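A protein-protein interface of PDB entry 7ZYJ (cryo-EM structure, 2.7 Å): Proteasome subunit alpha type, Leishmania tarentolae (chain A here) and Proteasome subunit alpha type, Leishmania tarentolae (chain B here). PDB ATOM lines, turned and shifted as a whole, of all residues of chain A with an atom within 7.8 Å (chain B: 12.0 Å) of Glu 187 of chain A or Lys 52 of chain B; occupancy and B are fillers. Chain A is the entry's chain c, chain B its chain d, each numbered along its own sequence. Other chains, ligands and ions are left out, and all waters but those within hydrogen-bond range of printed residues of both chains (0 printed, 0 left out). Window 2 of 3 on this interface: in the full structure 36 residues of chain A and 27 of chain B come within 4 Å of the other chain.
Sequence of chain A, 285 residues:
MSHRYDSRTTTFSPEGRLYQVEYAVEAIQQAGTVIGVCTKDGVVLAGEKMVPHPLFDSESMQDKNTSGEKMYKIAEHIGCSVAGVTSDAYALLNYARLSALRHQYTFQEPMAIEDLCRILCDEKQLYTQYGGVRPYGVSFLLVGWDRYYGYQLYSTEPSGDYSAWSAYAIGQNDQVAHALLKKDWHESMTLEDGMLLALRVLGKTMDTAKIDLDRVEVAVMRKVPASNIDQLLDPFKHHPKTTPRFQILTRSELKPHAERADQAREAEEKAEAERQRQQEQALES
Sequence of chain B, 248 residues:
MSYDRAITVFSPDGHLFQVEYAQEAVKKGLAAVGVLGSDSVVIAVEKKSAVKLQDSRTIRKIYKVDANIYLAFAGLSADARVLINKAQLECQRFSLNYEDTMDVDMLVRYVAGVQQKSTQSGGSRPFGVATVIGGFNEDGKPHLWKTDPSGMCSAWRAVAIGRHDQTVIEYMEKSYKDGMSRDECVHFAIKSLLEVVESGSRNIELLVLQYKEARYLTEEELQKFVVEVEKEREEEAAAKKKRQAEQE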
ATOM      1  N   CYS A  38      33.475   5.125  11.515  1.00  0.00           N
ATOM      2  CA  CYS A  38      33.640   3.927  10.694  1.00  0.00           C
ATOM      3  C   CYS A  38      34.706   4.207   9.640  1.00  0.00           C
ATOM      4  O   CYS A  38      34.446   4.882   8.642  1.00  0.00           O
ATOM      5  CB  CYS A  38      32.315   3.524  10.055  1.00  0.00           C
ATOM      6  SG  CYS A  38      32.319   1.892   9.281  1.00  0.00           S
ATOM      7  N   THR A  39      35.908   3.686   9.866  1.00  0.00           N
ATOM      8  CA  THR A  39      37.001   3.824   8.917  1.00  0.00           C
ATOM      9  C   THR A  39      37.036   2.597   8.004  1.00  0.00           C
ATOM     10  O   THR A  39      36.152   1.739   8.046  1.00  0.00           O
ATOM     11  CB  THR A  39      38.324   4.027   9.652  1.00  0.00           C
ATOM     12  OG1 THR A  39      38.754   2.784  10.220  1.00  0.00           O
ATOM     13  CG2 THR A  39      38.164   5.055  10.760  1.00  0.00           C
ATOM     14  N   LYS A  40      38.065   2.505   7.163  1.00  0.00           N
ATOM     15  CA  LYS A  40      38.206   1.390   6.238  1.00  0.00           C
ATOM     16  C   LYS A  40      38.975   0.217   6.830  1.00  0.00           C
ATOM     17  O   LYS A  40      38.888  -0.895   6.296  1.00  0.00           O
ATOM     18  CB  LYS A  40      38.895   1.863   4.949  1.00  0.00           C
ATOM     19  CG  LYS A  40      38.815   0.881   3.790  1.00  0.00           C
ATOM     20  CD  LYS A  40      37.374   0.602   3.400  1.00  0.00           C
ATOM     21  CE  LYS A  40      36.718   1.826   2.784  1.00  0.00           C
ATOM     22  NZ  LYS A  40      37.287   2.146   1.447  1.00  0.00           N
ATOM     23  N   ASP A  41      39.704   0.425   7.926  1.00  0.00           N
ATOM     24  CA  ASP A  41      40.456  -0.640   8.578  1.00  0.00           C
ATOM     25  C   ASP A  41      40.013  -0.815  10.025  1.00  0.00           C
ATOM     26  O   ASP A  41      40.820  -1.163  10.890  1.00  0.00           O
ATOM     27  CB  ASP A  41      41.957  -0.374   8.505  1.00  0.00           C
ATOM     28  CG  ASP A  41      42.319   1.034   8.928  1.00  0.00           C
ATOM     29  OD1 ASP A  41      41.394   1.836   9.175  1.00  0.00           O
ATOM     30  OD2 ASP A  41      43.527   1.339   9.017  1.00  0.00           O
ATOM     31  N   TRP A 165      25.737   4.780   9.198  1.00  0.00           N
ATOM     32  CA  TRP A 165      26.521   6.002   9.199  1.00  0.00           C
ATOM     33  C   TRP A 165      27.995   5.681   8.997  1.00  0.00           C
ATOM     34  O   TRP A 165      28.481   4.613   9.371  1.00  0.00           O
ATOM     35  CB  TRP A 165      26.344   6.781  10.510  1.00  0.00           C
ATOM     36  CG  TRP A 165      24.921   7.091  10.837  1.00  0.00           C
ATOM     37  CD1 TRP A 165      24.107   6.401  11.687  1.00  0.00           C
ATOM     38  CD2 TRP A 165      24.137   8.172  10.321  1.00  0.00           C
ATOM     39  NE1 TRP A 165      22.866   6.985  11.732  1.00  0.00           N
ATOM     40  CE2 TRP A 165      22.858   8.074  10.901  1.00  0.00           C
ATOM     41  CE3 TRP A 165      24.392   9.213   9.425  1.00  0.00           C
ATOM     42  CZ2 TRP A 165      21.838   8.977  10.615  1.00  0.00           C
ATOM     43  CZ3 TRP A 165      23.379  10.107   9.140  1.00  0.00           C
ATOM     44  CH2 TRP A 165      22.117   9.984   9.734  1.00  0.00           C
ATOM     45  N   SER A 166      28.700   6.632   8.385  1.00  0.00           N
ATOM     46  CA  SER A 166      30.154   6.611   8.368  1.00  0.00           C
ATOM     47  C   SER A 166      30.743   7.172   9.652  1.00  0.00           C
ATOM     48  O   SER A 166      31.818   6.736  10.082  1.00  0.00           O
ATOM     49  CB  SER A 166      30.679   7.406   7.170  1.00  0.00           C
ATOM     50  OG  SER A 166      30.360   6.761   5.950  1.00  0.00           O
ATOM     51  N   ALA A 167      30.056   8.131  10.267  1.00  0.00           N
ATOM     52  CA  ALA A 167      30.438   8.674  11.564  1.00  0.00           C
ATOM     53  C   ALA A 167      29.196   9.286  12.188  1.00  0.00           C
ATOM     54  O   ALA A 167      28.458  10.009  11.513  1.00  0.00           O
ATOM     55  CB  ALA A 167      31.550   9.718  11.430  1.00  0.00           C
ATOM     56  N   LEU A 181      32.026  16.286  13.332  1.00  0.00           N
ATOM     57  CA  LEU A 181      32.400  15.122  12.535  1.00  0.00           C
ATOM     58  C   LEU A 181      32.267  15.399  11.044  1.00  0.00           C
ATOM     59  O   LEU A 181      33.044  14.867  10.245  1.00  0.00           O
ATOM     60  CB  LEU A 181      31.546  13.916  12.927  1.00  0.00           C
ATOM     61  CG  LEU A 181      31.891  13.220  14.243  1.00  0.00           C
ATOM     62  CD1 LEU A 181      30.773  12.276  14.650  1.00  0.00           C
ATOM     63  CD2 LEU A 181      33.209  12.475  14.124  1.00  0.00           C
ATOM     64  N   LYS A 182      31.288  16.217  10.654  1.00  0.00           N
ATOM     65  CA  LYS A 182      31.137  16.578   9.249  1.00  0.00           C
ATOM     66  C   LYS A 182      32.312  17.412   8.756  1.00  0.00           C
ATOM     67  O   LYS A 182      32.713  17.289   7.593  1.00  0.00           O
ATOM     68  CB  LYS A 182      29.825  17.333   9.043  1.00  0.00           C
ATOM     69  CG  LYS A 182      29.453  17.559   7.588  1.00  0.00           C
ATOM     70  CD  LYS A 182      28.197  18.407   7.472  1.00  0.00           C
ATOM     71  CE  LYS A 182      26.967  17.633   7.917  1.00  0.00           C
ATOM     72  NZ  LYS A 182      25.717  18.418   7.729  1.00  0.00           N
ATOM     73  N   LYS A 183      32.869  18.264   9.619  1.00  0.00           N
ATOM     74  CA  LYS A 183      34.003  19.094   9.226  1.00  0.00           C
ATOM     75  C   LYS A 183      35.213  18.243   8.863  1.00  0.00           C
ATOM     76  O   LYS A 183      35.909  18.519   7.880  1.00  0.00           O
ATOM     77  CB  LYS A 183      34.355  20.067  10.351  1.00  0.00           C
ATOM     78  CG  LYS A 183      33.251  21.048  10.710  1.00  0.00           C
ATOM     79  CD  LYS A 183      32.993  22.031   9.582  1.00  0.00           C
ATOM     80  CE  LYS A 183      31.943  23.057   9.977  1.00  0.00           C
ATOM     81  NZ  LYS A 183      31.643  24.006   8.870  1.00  0.00           N
ATOM     82  N   ASP A 184      35.480  17.201   9.645  1.00  0.00           N
ATOM     83  CA  ASP A 184      36.692  16.397   9.506  1.00  0.00           C
ATOM     84  C   ASP A 184      36.318  14.923   9.383  1.00  0.00           C
ATOM     85  O   ASP A 184      36.240  14.208  10.384  1.00  0.00           O
ATOM     86  CB  ASP A 184      37.629  16.628  10.691  1.00  0.00           C
ATOM     87  CG  ASP A 184      38.075  18.070  10.808  1.00  0.00           C
ATOM     88  OD1 ASP A 184      38.135  18.762   9.771  1.00  0.00           O
ATOM     89  OD2 ASP A 184      38.367  18.511  11.939  1.00  0.00           O
ATOM     90  N   TRP A 185      36.089  14.466   8.153  1.00  0.00           N
ATOM     91  CA  TRP A 185      35.970  13.038   7.891  1.00  0.00           C
ATOM     92  C   TRP A 185      36.184  12.796   6.407  1.00  0.00           C
ATOM     93  O   TRP A 185      35.657  13.539   5.574  1.00  0.00           O
ATOM     94  CB  TRP A 185      34.609  12.478   8.322  1.00  0.00           C
ATOM     95  CG  TRP A 185      34.569  10.981   8.244  1.00  0.00           C
ATOM     96  CD1 TRP A 185      34.913  10.102   9.229  1.00  0.00           C
ATOM     97  CD2 TRP A 185      34.204  10.188   7.109  1.00  0.00           C
ATOM     98  NE1 TRP A 185      34.767   8.810   8.784  1.00  0.00           N
ATOM     99  CE2 TRP A 185      34.333   8.836   7.484  1.00  0.00           C
ATOM    100  CE3 TRP A 185      33.772  10.489   5.814  1.00  0.00           C
ATOM    101  CZ2 TRP A 185      34.049   7.789   6.612  1.00  0.00           C
ATOM    102  CZ3 TRP A 185      33.487   9.446   4.950  1.00  0.00           C
ATOM    103  CH2 TRP A 185      33.626   8.114   5.354  1.00  0.00           C
ATOM    104  N   HIS A 186      36.958  11.762   6.083  1.00  0.00           N
ATOM    105  CA  HIS A 186      37.209  11.380   4.704  1.00  0.00           C
ATOM    106  C   HIS A 186      37.296   9.864   4.616  1.00  0.00           C
ATOM    107  O   HIS A 186      37.598   9.180   5.597  1.00  0.00           O
ATOM    108  CB  HIS A 186      38.491  12.027   4.163  1.00  0.00           C
ATOM    109  CG  HIS A 186      39.631  12.014   5.132  1.00  0.00           C
ATOM    110  ND1 HIS A 186      40.566  11.003   5.169  1.00  0.00           N
ATOM    111  CD2 HIS A 186      39.987  12.891   6.101  1.00  0.00           C
ATOM    112  CE1 HIS A 186      41.449  11.256   6.119  1.00  0.00           C
ATOM    113  NE2 HIS A 186      41.120  12.396   6.700  1.00  0.00           N
ATOM    114  N   GLU A 187      37.018   9.343   3.419  1.00  0.00           N
ATOM    115  CA  GLU A 187      37.046   7.897   3.218  1.00  0.00           C
ATOM    116  C   GLU A 187      38.462   7.343   3.308  1.00  0.00           C
ATOM    117  O   GLU A 187      38.651   6.207   3.757  1.00  0.00           O
ATOM    118  CB  GLU A 187      36.420   7.532   1.869  1.00  0.00           C
ATOM    119  CG  GLU A 187      35.011   8.076   1.639  1.00  0.00           C
ATOM    120  CD  GLU A 187      34.986   9.546   1.258  1.00  0.00           C
ATOM    121  OE1 GLU A 187      33.879  10.109   1.129  1.00  0.00           O
ATOM    122  OE2 GLU A 187      36.073  10.138   1.087  1.00  0.00           O
ATOM    123  N   SER A 188      39.462   8.120   2.891  1.00  0.00           N
ATOM    124  CA  SER A 188      40.860   7.697   2.966  1.00  0.00           C
ATOM    125  C   SER A 188      41.437   8.009   4.349  1.00  0.00           C
ATOM    126  O   SER A 188      42.368   8.795   4.514  1.00  0.00           O
ATOM    127  CB  SER A 188      41.669   8.365   1.862  1.00  0.00           C
ATOM    128  OG  SER A 188      43.042   8.033   1.962  1.00  0.00           O
ATOM    129  N   MET A 189      40.857   7.362   5.357  1.00  0.00           N
ATOM    130  CA  MET A 189      41.211   7.595   6.752  1.00  0.00           C
ATOM    131  C   MET A 189      41.610   6.273   7.387  1.00  0.00           C
ATOM    132  O   MET A 189      40.876   5.286   7.283  1.00  0.00           O
ATOM    133  CB  MET A 189      40.043   8.231   7.510  1.00  0.00           C
ATOM    134  CG  MET A 189      40.278   8.425   8.993  1.00  0.00           C
ATOM    135  SD  MET A 189      38.805   9.063   9.813  1.00  0.00           S
ATOM    136  CE  MET A 189      38.601  10.626   8.965  1.00  0.00           C
ATOM    137  N   THR A 190      42.770   6.256   8.042  1.00  0.00           N
ATOM    138  CA  THR A 190      43.253   5.051   8.696  1.00  0.00           C
ATOM    139  C   THR A 190      42.567   4.872  10.049  1.00  0.00           C
ATOM    140  O   THR A 190      41.828   5.739  10.525  1.00  0.00           O
ATOM    141  CB  THR A 190      44.770   5.105   8.861  1.00  0.00           C
ATOM    142  OG1 THR A 190      45.110   6.095   9.840  1.00  0.00           O
ATOM    143  CG2 THR A 190      45.437   5.456   7.540  1.00  0.00           C
ATOM    144  N   LYS B  47      14.131  10.514  -0.750  1.00  0.00           N
ATOM    145  CA  LYS B  47      15.548  10.254  -0.485  1.00  0.00           C
ATOM    146  C   LYS B  47      16.172  11.418   0.292  1.00  0.00           C
ATOM    147  O   LYS B  47      17.006  12.169  -0.215  1.00  0.00           O
ATOM    148  CB  LYS B  47      16.302   9.982  -1.791  1.00  0.00           C
ATOM    149  CG  LYS B  47      17.686   9.384  -1.597  1.00  0.00           C
ATOM    150  CD  LYS B  47      18.422   9.253  -2.921  1.00  0.00           C
ATOM    151  CE  LYS B  47      19.907   9.526  -2.756  1.00  0.00           C
ATOM    152  NZ  LYS B  47      20.167  10.927  -2.323  1.00  0.00           N
ATOM    153  N   LYS B  48      15.736  11.531   1.548  1.00  0.00           N
ATOM    154  CA  LYS B  48      15.737  12.767   2.330  1.00  0.00           C
ATOM    155  C   LYS B  48      16.892  13.717   2.041  1.00  0.00           C
ATOM    156  O   LYS B  48      16.655  14.881   1.700  1.00  0.00           O
ATOM    157  CB  LYS B  48      15.746  12.418   3.822  1.00  0.00           C
ATOM    158  CG  LYS B  48      15.879  13.615   4.746  1.00  0.00           C
ATOM    159  CD  LYS B  48      15.319  13.309   6.126  1.00  0.00           C
ATOM    160  CE  LYS B  48      14.942  14.581   6.863  1.00  0.00           C
ATOM    161  NZ  LYS B  48      14.242  15.551   5.976  1.00  0.00           N
ATOM    162  N   SER B  49      18.136  13.244   2.146  1.00  0.00           N
ATOM    163  CA  SER B  49      19.288  14.101   1.882  1.00  0.00           C
ATOM    164  C   SER B  49      20.595  13.321   1.864  1.00  0.00           C
ATOM    165  O   SER B  49      20.623  12.124   2.166  1.00  0.00           O
ATOM    166  CB  SER B  49      19.390  15.219   2.928  1.00  0.00           C
ATOM    167  OG  SER B  49      18.346  16.165   2.782  1.00  0.00           O
ATOM    168  N   ALA B  50      21.683  14.002   1.508  1.00  0.00           N
ATOM    169  CA  ALA B  50      23.034  13.480   1.658  1.00  0.00           C
ATOM    170  C   ALA B  50      23.671  14.201   2.840  1.00  0.00           C
ATOM    171  O   ALA B  50      24.069  15.366   2.726  1.00  0.00           O
ATOM    172  CB  ALA B  50      23.848  13.677   0.382  1.00  0.00           C
ATOM    173  N   VAL B  51      23.767  13.505   3.977  1.00  0.00           N
ATOM    174  CA  VAL B  51      24.211  14.129   5.220  1.00  0.00           C
ATOM    175  C   VAL B  51      25.728  14.247   5.297  1.00  0.00           C
ATOM    176  O   VAL B  51      26.240  14.966   6.170  1.00  0.00           O
ATOM    177  CB  VAL B  51      23.624  13.325   6.404  1.00  0.00           C
ATOM    178  CG1 VAL B  51      24.030  13.905   7.757  1.00  0.00           C
ATOM    179  CG2 VAL B  51      22.109  13.256   6.293  1.00  0.00           C
ATOM    180  N   LYS B  52      26.461  13.582   4.394  1.00  0.00           N
ATOM    181  CA  LYS B  52      27.924  13.529   4.372  1.00  0.00           C
ATOM    182  C   LYS B  52      28.406  12.627   5.507  1.00  0.00           C
ATOM    183  O   LYS B  52      29.589  12.278   5.588  1.00  0.00           O
ATOM    184  CB  LYS B  52      28.524  14.947   4.442  1.00  0.00           C
ATOM    185  CG  LYS B  52      30.020  15.061   4.717  1.00  0.00           C
ATOM    186  CD  LYS B  52      30.847  14.413   3.619  1.00  0.00           C
ATOM    187  CE  LYS B  52      32.132  13.821   4.178  1.00  0.00           C
ATOM    188  NZ  LYS B  52      32.669  12.737   3.312  1.00  0.00           N
ATOM    189  N   LEU B  53      27.476  12.185   6.354  1.00  0.00           N
ATOM    190  CA  LEU B  53      27.773  11.243   7.418  1.00  0.00           C
ATOM    191  C   LEU B  53      27.162   9.871   7.189  1.00  0.00           C
ATOM    192  O   LEU B  53      27.527   8.926   7.898  1.00  0.00           O
ATOM    193  CB  LEU B  53      27.288  11.791   8.770  1.00  0.00           C
ATOM    194  CG  LEU B  53      28.153  12.893   9.380  1.00  0.00           C
ATOM    195  CD1 LEU B  53      27.560  13.379  10.694  1.00  0.00           C
ATOM    196  CD2 LEU B  53      29.582  12.410   9.574  1.00  0.00           C
ATOM    197  N   GLN B  54      26.250   9.731   6.229  1.00  0.00           N
ATOM    198  CA  GLN B  54      25.702   8.426   5.899  1.00  0.00           C
ATOM    199  C   GLN B  54      26.773   7.549   5.256  1.00  0.00           C
ATOM    200  O   GLN B  54      27.793   8.030   4.756  1.00  0.00           O
ATOM    201  CB  GLN B  54      24.508   8.561   4.956  1.00  0.00           C
ATOM    202  CG  GLN B  54      23.309   9.276   5.551  1.00  0.00           C
ATOM    203  CD  GLN B  54      22.312   9.707   4.494  1.00  0.00           C
ATOM    204  OE1 GLN B  54      21.407  10.496   4.762  1.00  0.00           O
ATOM    205  NE2 GLN B  54      22.474   9.188   3.282  1.00  0.00           N
ATOM    206  N   ASP B  55      26.525   6.243   5.279  1.00  0.00           N
ATOM    207  CA  ASP B  55      27.462   5.293   4.699  1.00  0.00           C
ATOM    208  C   ASP B  55      27.583   5.508   3.196  1.00  0.00           C
ATOM    209  O   ASP B  55      26.606   5.834   2.516  1.00  0.00           O
ATOM    210  CB  ASP B  55      27.013   3.863   4.990  1.00  0.00           C
ATOM    211  CG  ASP B  55      28.157   2.873   4.947  1.00  0.00           C
ATOM    212  OD1 ASP B  55      29.308   3.301   4.729  1.00  0.00           O
ATOM    213  OD2 ASP B  55      27.904   1.663   5.129  1.00  0.00           O
ATOM    214  N   SER B  56      28.803   5.331   2.678  1.00  0.00           N
ATOM    215  CA  SER B  56      29.021   5.452   1.240  1.00  0.00           C
ATOM    216  C   SER B  56      28.241   4.398   0.469  1.00  0.00           C
ATOM    217  O   SER B  56      27.790   4.657  -0.653  1.00  0.00           O
ATOM    218  CB  SER B  56      30.513   5.350   0.923  1.00  0.00           C
ATOM    219  OG  SER B  56      31.239   6.403   1.535  1.00  0.00           O
ATOM    220  N   ARG B  57      28.086   3.207   1.043  1.00  0.00           N
ATOM    221  CA  ARG B  57      27.251   2.181   0.438  1.00  0.00           C
ATOM    222  C   ARG B  57      25.827   2.691   0.262  1.00  0.00           C
ATOM    223  O   ARG B  57      25.256   3.314   1.160  1.00  0.00           O
ATOM    224  CB  ARG B  57      27.257   0.921   1.304  1.00  0.00           C
ATOM    225  CG  ARG B  57      25.961   0.130   1.262  1.00  0.00           C
ATOM    226  CD  ARG B  57      26.081  -1.163   2.041  1.00  0.00           C
ATOM    227  NE  ARG B  57      25.969  -0.952   3.479  1.00  0.00           N
ATOM    228  CZ  ARG B  57      24.922  -1.307   4.210  1.00  0.00           C
ATOM    229  NH1 ARG B  57      23.868  -1.893   3.667  1.00  0.00           N
ATOM    230  NH2 ARG B  57      24.932  -1.068   5.518  1.00  0.00           N
ATOM    231  N   THR B  58      25.255   2.429  -0.909  1.00  0.00           N
ATOM    232  CA  THR B  58      23.901   2.872  -1.198  1.00  0.00           C
ATOM    233  C   THR B  58      22.881   1.936  -0.564  1.00  0.00           C
ATOM    234  O   THR B  58      23.068   0.716  -0.525  1.00  0.00           O
ATOM    235  CB  THR B  58      23.674   2.965  -2.710  1.00  0.00           C
ATOM    236  OG1 THR B  58      22.374   3.510  -2.969  1.00  0.00           O
ATOM    237  CG2 THR B  58      23.797   1.599  -3.376  1.00  0.00           C
ATOM    238  N   LYS B  61      15.549   3.190  -0.806  1.00  0.00           N
ATOM    239  CA  LYS B  61      14.321   3.570  -0.125  1.00  0.00           C
ATOM    240  C   LYS B  61      13.083   2.976  -0.779  1.00  0.00           C
ATOM    241  O   LYS B  61      11.977   3.158  -0.259  1.00  0.00           O
ATOM    242  CB  LYS B  61      14.192   5.097  -0.068  1.00  0.00           C
ATOM    243  CG  LYS B  61      15.327   5.781   0.672  1.00  0.00           C
ATOM    244  CD  LYS B  61      15.399   5.310   2.115  1.00  0.00           C
ATOM    245  CE  LYS B  61      16.474   6.056   2.887  1.00  0.00           C
ATOM    246  NZ  LYS B  61      17.840   5.696   2.419  1.00  0.00           N
ATOM    247  N   ARG B 202      20.391  15.618  -5.649  1.00  0.00           N
ATOM    248  CA  ARG B 202      20.866  14.484  -4.864  1.00  0.00           C
ATOM    249  C   ARG B 202      19.827  13.999  -3.857  1.00  0.00           C
ATOM    250  O   ARG B 202      20.162  13.279  -2.909  1.00  0.00           O
ATOM    251  CB  ARG B 202      22.184  14.840  -4.167  1.00  0.00           C
ATOM    252  CG  ARG B 202      22.077  15.669  -2.882  1.00  0.00           C
ATOM    253  CD  ARG B 202      21.602  17.092  -3.141  1.00  0.00           C
ATOM    254  NE  ARG B 202      21.591  17.894  -1.924  1.00  0.00           N
ATOM    255  CZ  ARG B 202      20.603  17.907  -1.040  1.00  0.00           C
ATOM    256  NH1 ARG B 202      19.520  17.165  -1.204  1.00  0.00           N
ATOM    257  NH2 ARG B 202      20.706  18.681   0.037  1.00  0.00           N
ATOM    258  N   ASN B 203      18.561  14.356  -4.062  1.00  0.00           N
ATOM    259  CA  ASN B 203      17.463  13.978  -3.176  1.00  0.00           C
ATOM    260  C   ASN B 203      16.292  13.407  -3.978  1.00  0.00           C
ATOM    261  O   ASN B 203      15.123  13.718  -3.754  1.00  0.00           O
ATOM    262  CB  ASN B 203      17.108  15.171  -2.276  1.00  0.00           C
ATOM    263  CG  ASN B 203      16.396  16.306  -3.009  1.00  0.00           C
ATOM    264  OD1 ASN B 203      16.932  17.394  -3.205  1.00  0.00           O
ATOM    265  ND2 ASN B 203      15.166  16.037  -3.429  1.00  0.00           N
ATOM    266  N   GLU B 219      23.268   7.688 -10.722  1.00  0.00           N
ATOM    267  CA  GLU B 219      23.220   9.110 -10.395  1.00  0.00           C
ATOM    268  C   GLU B 219      23.346   9.975 -11.644  1.00  0.00           C
ATOM    269  O   GLU B 219      22.641  10.980 -11.778  1.00  0.00           O
ATOM    270  CB  GLU B 219      24.313   9.454  -9.384  1.00  0.00           C
ATOM    271  CG  GLU B 219      24.157   8.751  -8.043  1.00  0.00           C
ATOM    272  CD  GLU B 219      23.181   9.453  -7.114  1.00  0.00           C
ATOM    273  OE1 GLU B 219      22.390  10.292  -7.593  1.00  0.00           O
ATOM    274  OE2 GLU B 219      23.207   9.165  -5.899  1.00  0.00           O
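Of the 16 printed residues of chain B, 6 touch a printed residue of chain A.
Hydrophobic or aromatic side chains of chain B that line the printed part of chain A: Leu 53.
Of the 17 printed residues of chain A, 6 touch a printed residue of chain B.
Printed residues of chain A that touch a printed residue of chain B: Trp 165, Ser 166, Ala 167, Lys 182, Trp 185 and Glu 187.
Hydrophobic or aromatic side chains of chain A within 4 Å of the printed part of chain B: Trp 165, Ala 167 and Trp 185.
The backbone NH (N) of Ser 166 of chain A sits at hydrogen-bond distance from the backbone carbonyl oxygen (O) of Leu 53 of chain B (2.6 Å).
OG of Ser 166 of chain A lies within hydrogen-bond range of O of Gln 54 of chain B (3.1 Å).
OE1 of Glu 187 of chain A lies within salt-bridge range of NZ of Lys 52 of chain B (3.6 Å).
N of Cys 38 of chain A is in hydrogen-bond range of O of Ser 166 of chain A (2.7 Å).
The backbone carbonyl oxygen of Ser 49 of chain B lies close to the side-chain amide oxygen of Gln 54 of chain B.
The side-chain carboxylate (OD2) of Asp 55 of chain B lies within salt-bridge range of the guanidinium group (NE) of Arg 57 of chain B (3.6 Å).
No residue of chain B comes within 4 Å of Thr 39 of chain A.
Printed residues of chain B within 4 Å of Trp 165 of chain A: Leu 53 (3.4 Å), Gln 54 (3.7 Å) and Asp 55 (3.9 Å).
Lys 183 of chain A touches none of the printed residues of chain B.
His 186 of chain A touches none of the printed residues of chain B.
Glu 187 of chain A touches one residue of chain B.
No residue of chain B comes within 4 Å of Ser 188 of chain A.
No residue of chain B comes within 4 Å of Met 189 of chain A.
Lys 52 of chain B touches three residues of chain A.
Of the printed residues of chain A, Leu 53 of chain B touches Trp 165, Ser 166 and Ala 167.
Asn 203 of chain B touches none of the printed residues of chain A.
The nearest printed residue of chain A that does not touch Asp 55 of chain B is Cys 38 of chain A (5.6 Å).
O of Leu 53 of chain B touches CA of Trp 165 of chain A (3.4 Å).
Gln 54 of chain B touches Trp 165 of chain A.
Trp 165 of chain A touches Asp 55 of chain B (CA to N, 3.9 Å).
Ser 166 of chain A touches Asp 55 of chain B.
Ser 56 of chain B touches Ser 166 of chain A (N to OG, 3.9 Å).
CD2 of Leu 53 of chain B touches O of Ala 167 of chain A (3.3 Å).
Lys 182 of chain A touches Val 51 of chain B.
Lys 52 of chain B touches Lys 182 of chain A (CG to CG, 3.8 Å).
Trp 185 of chain A touches Lys 52 of chain B (CE3 to NZ, 3.5 Å).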
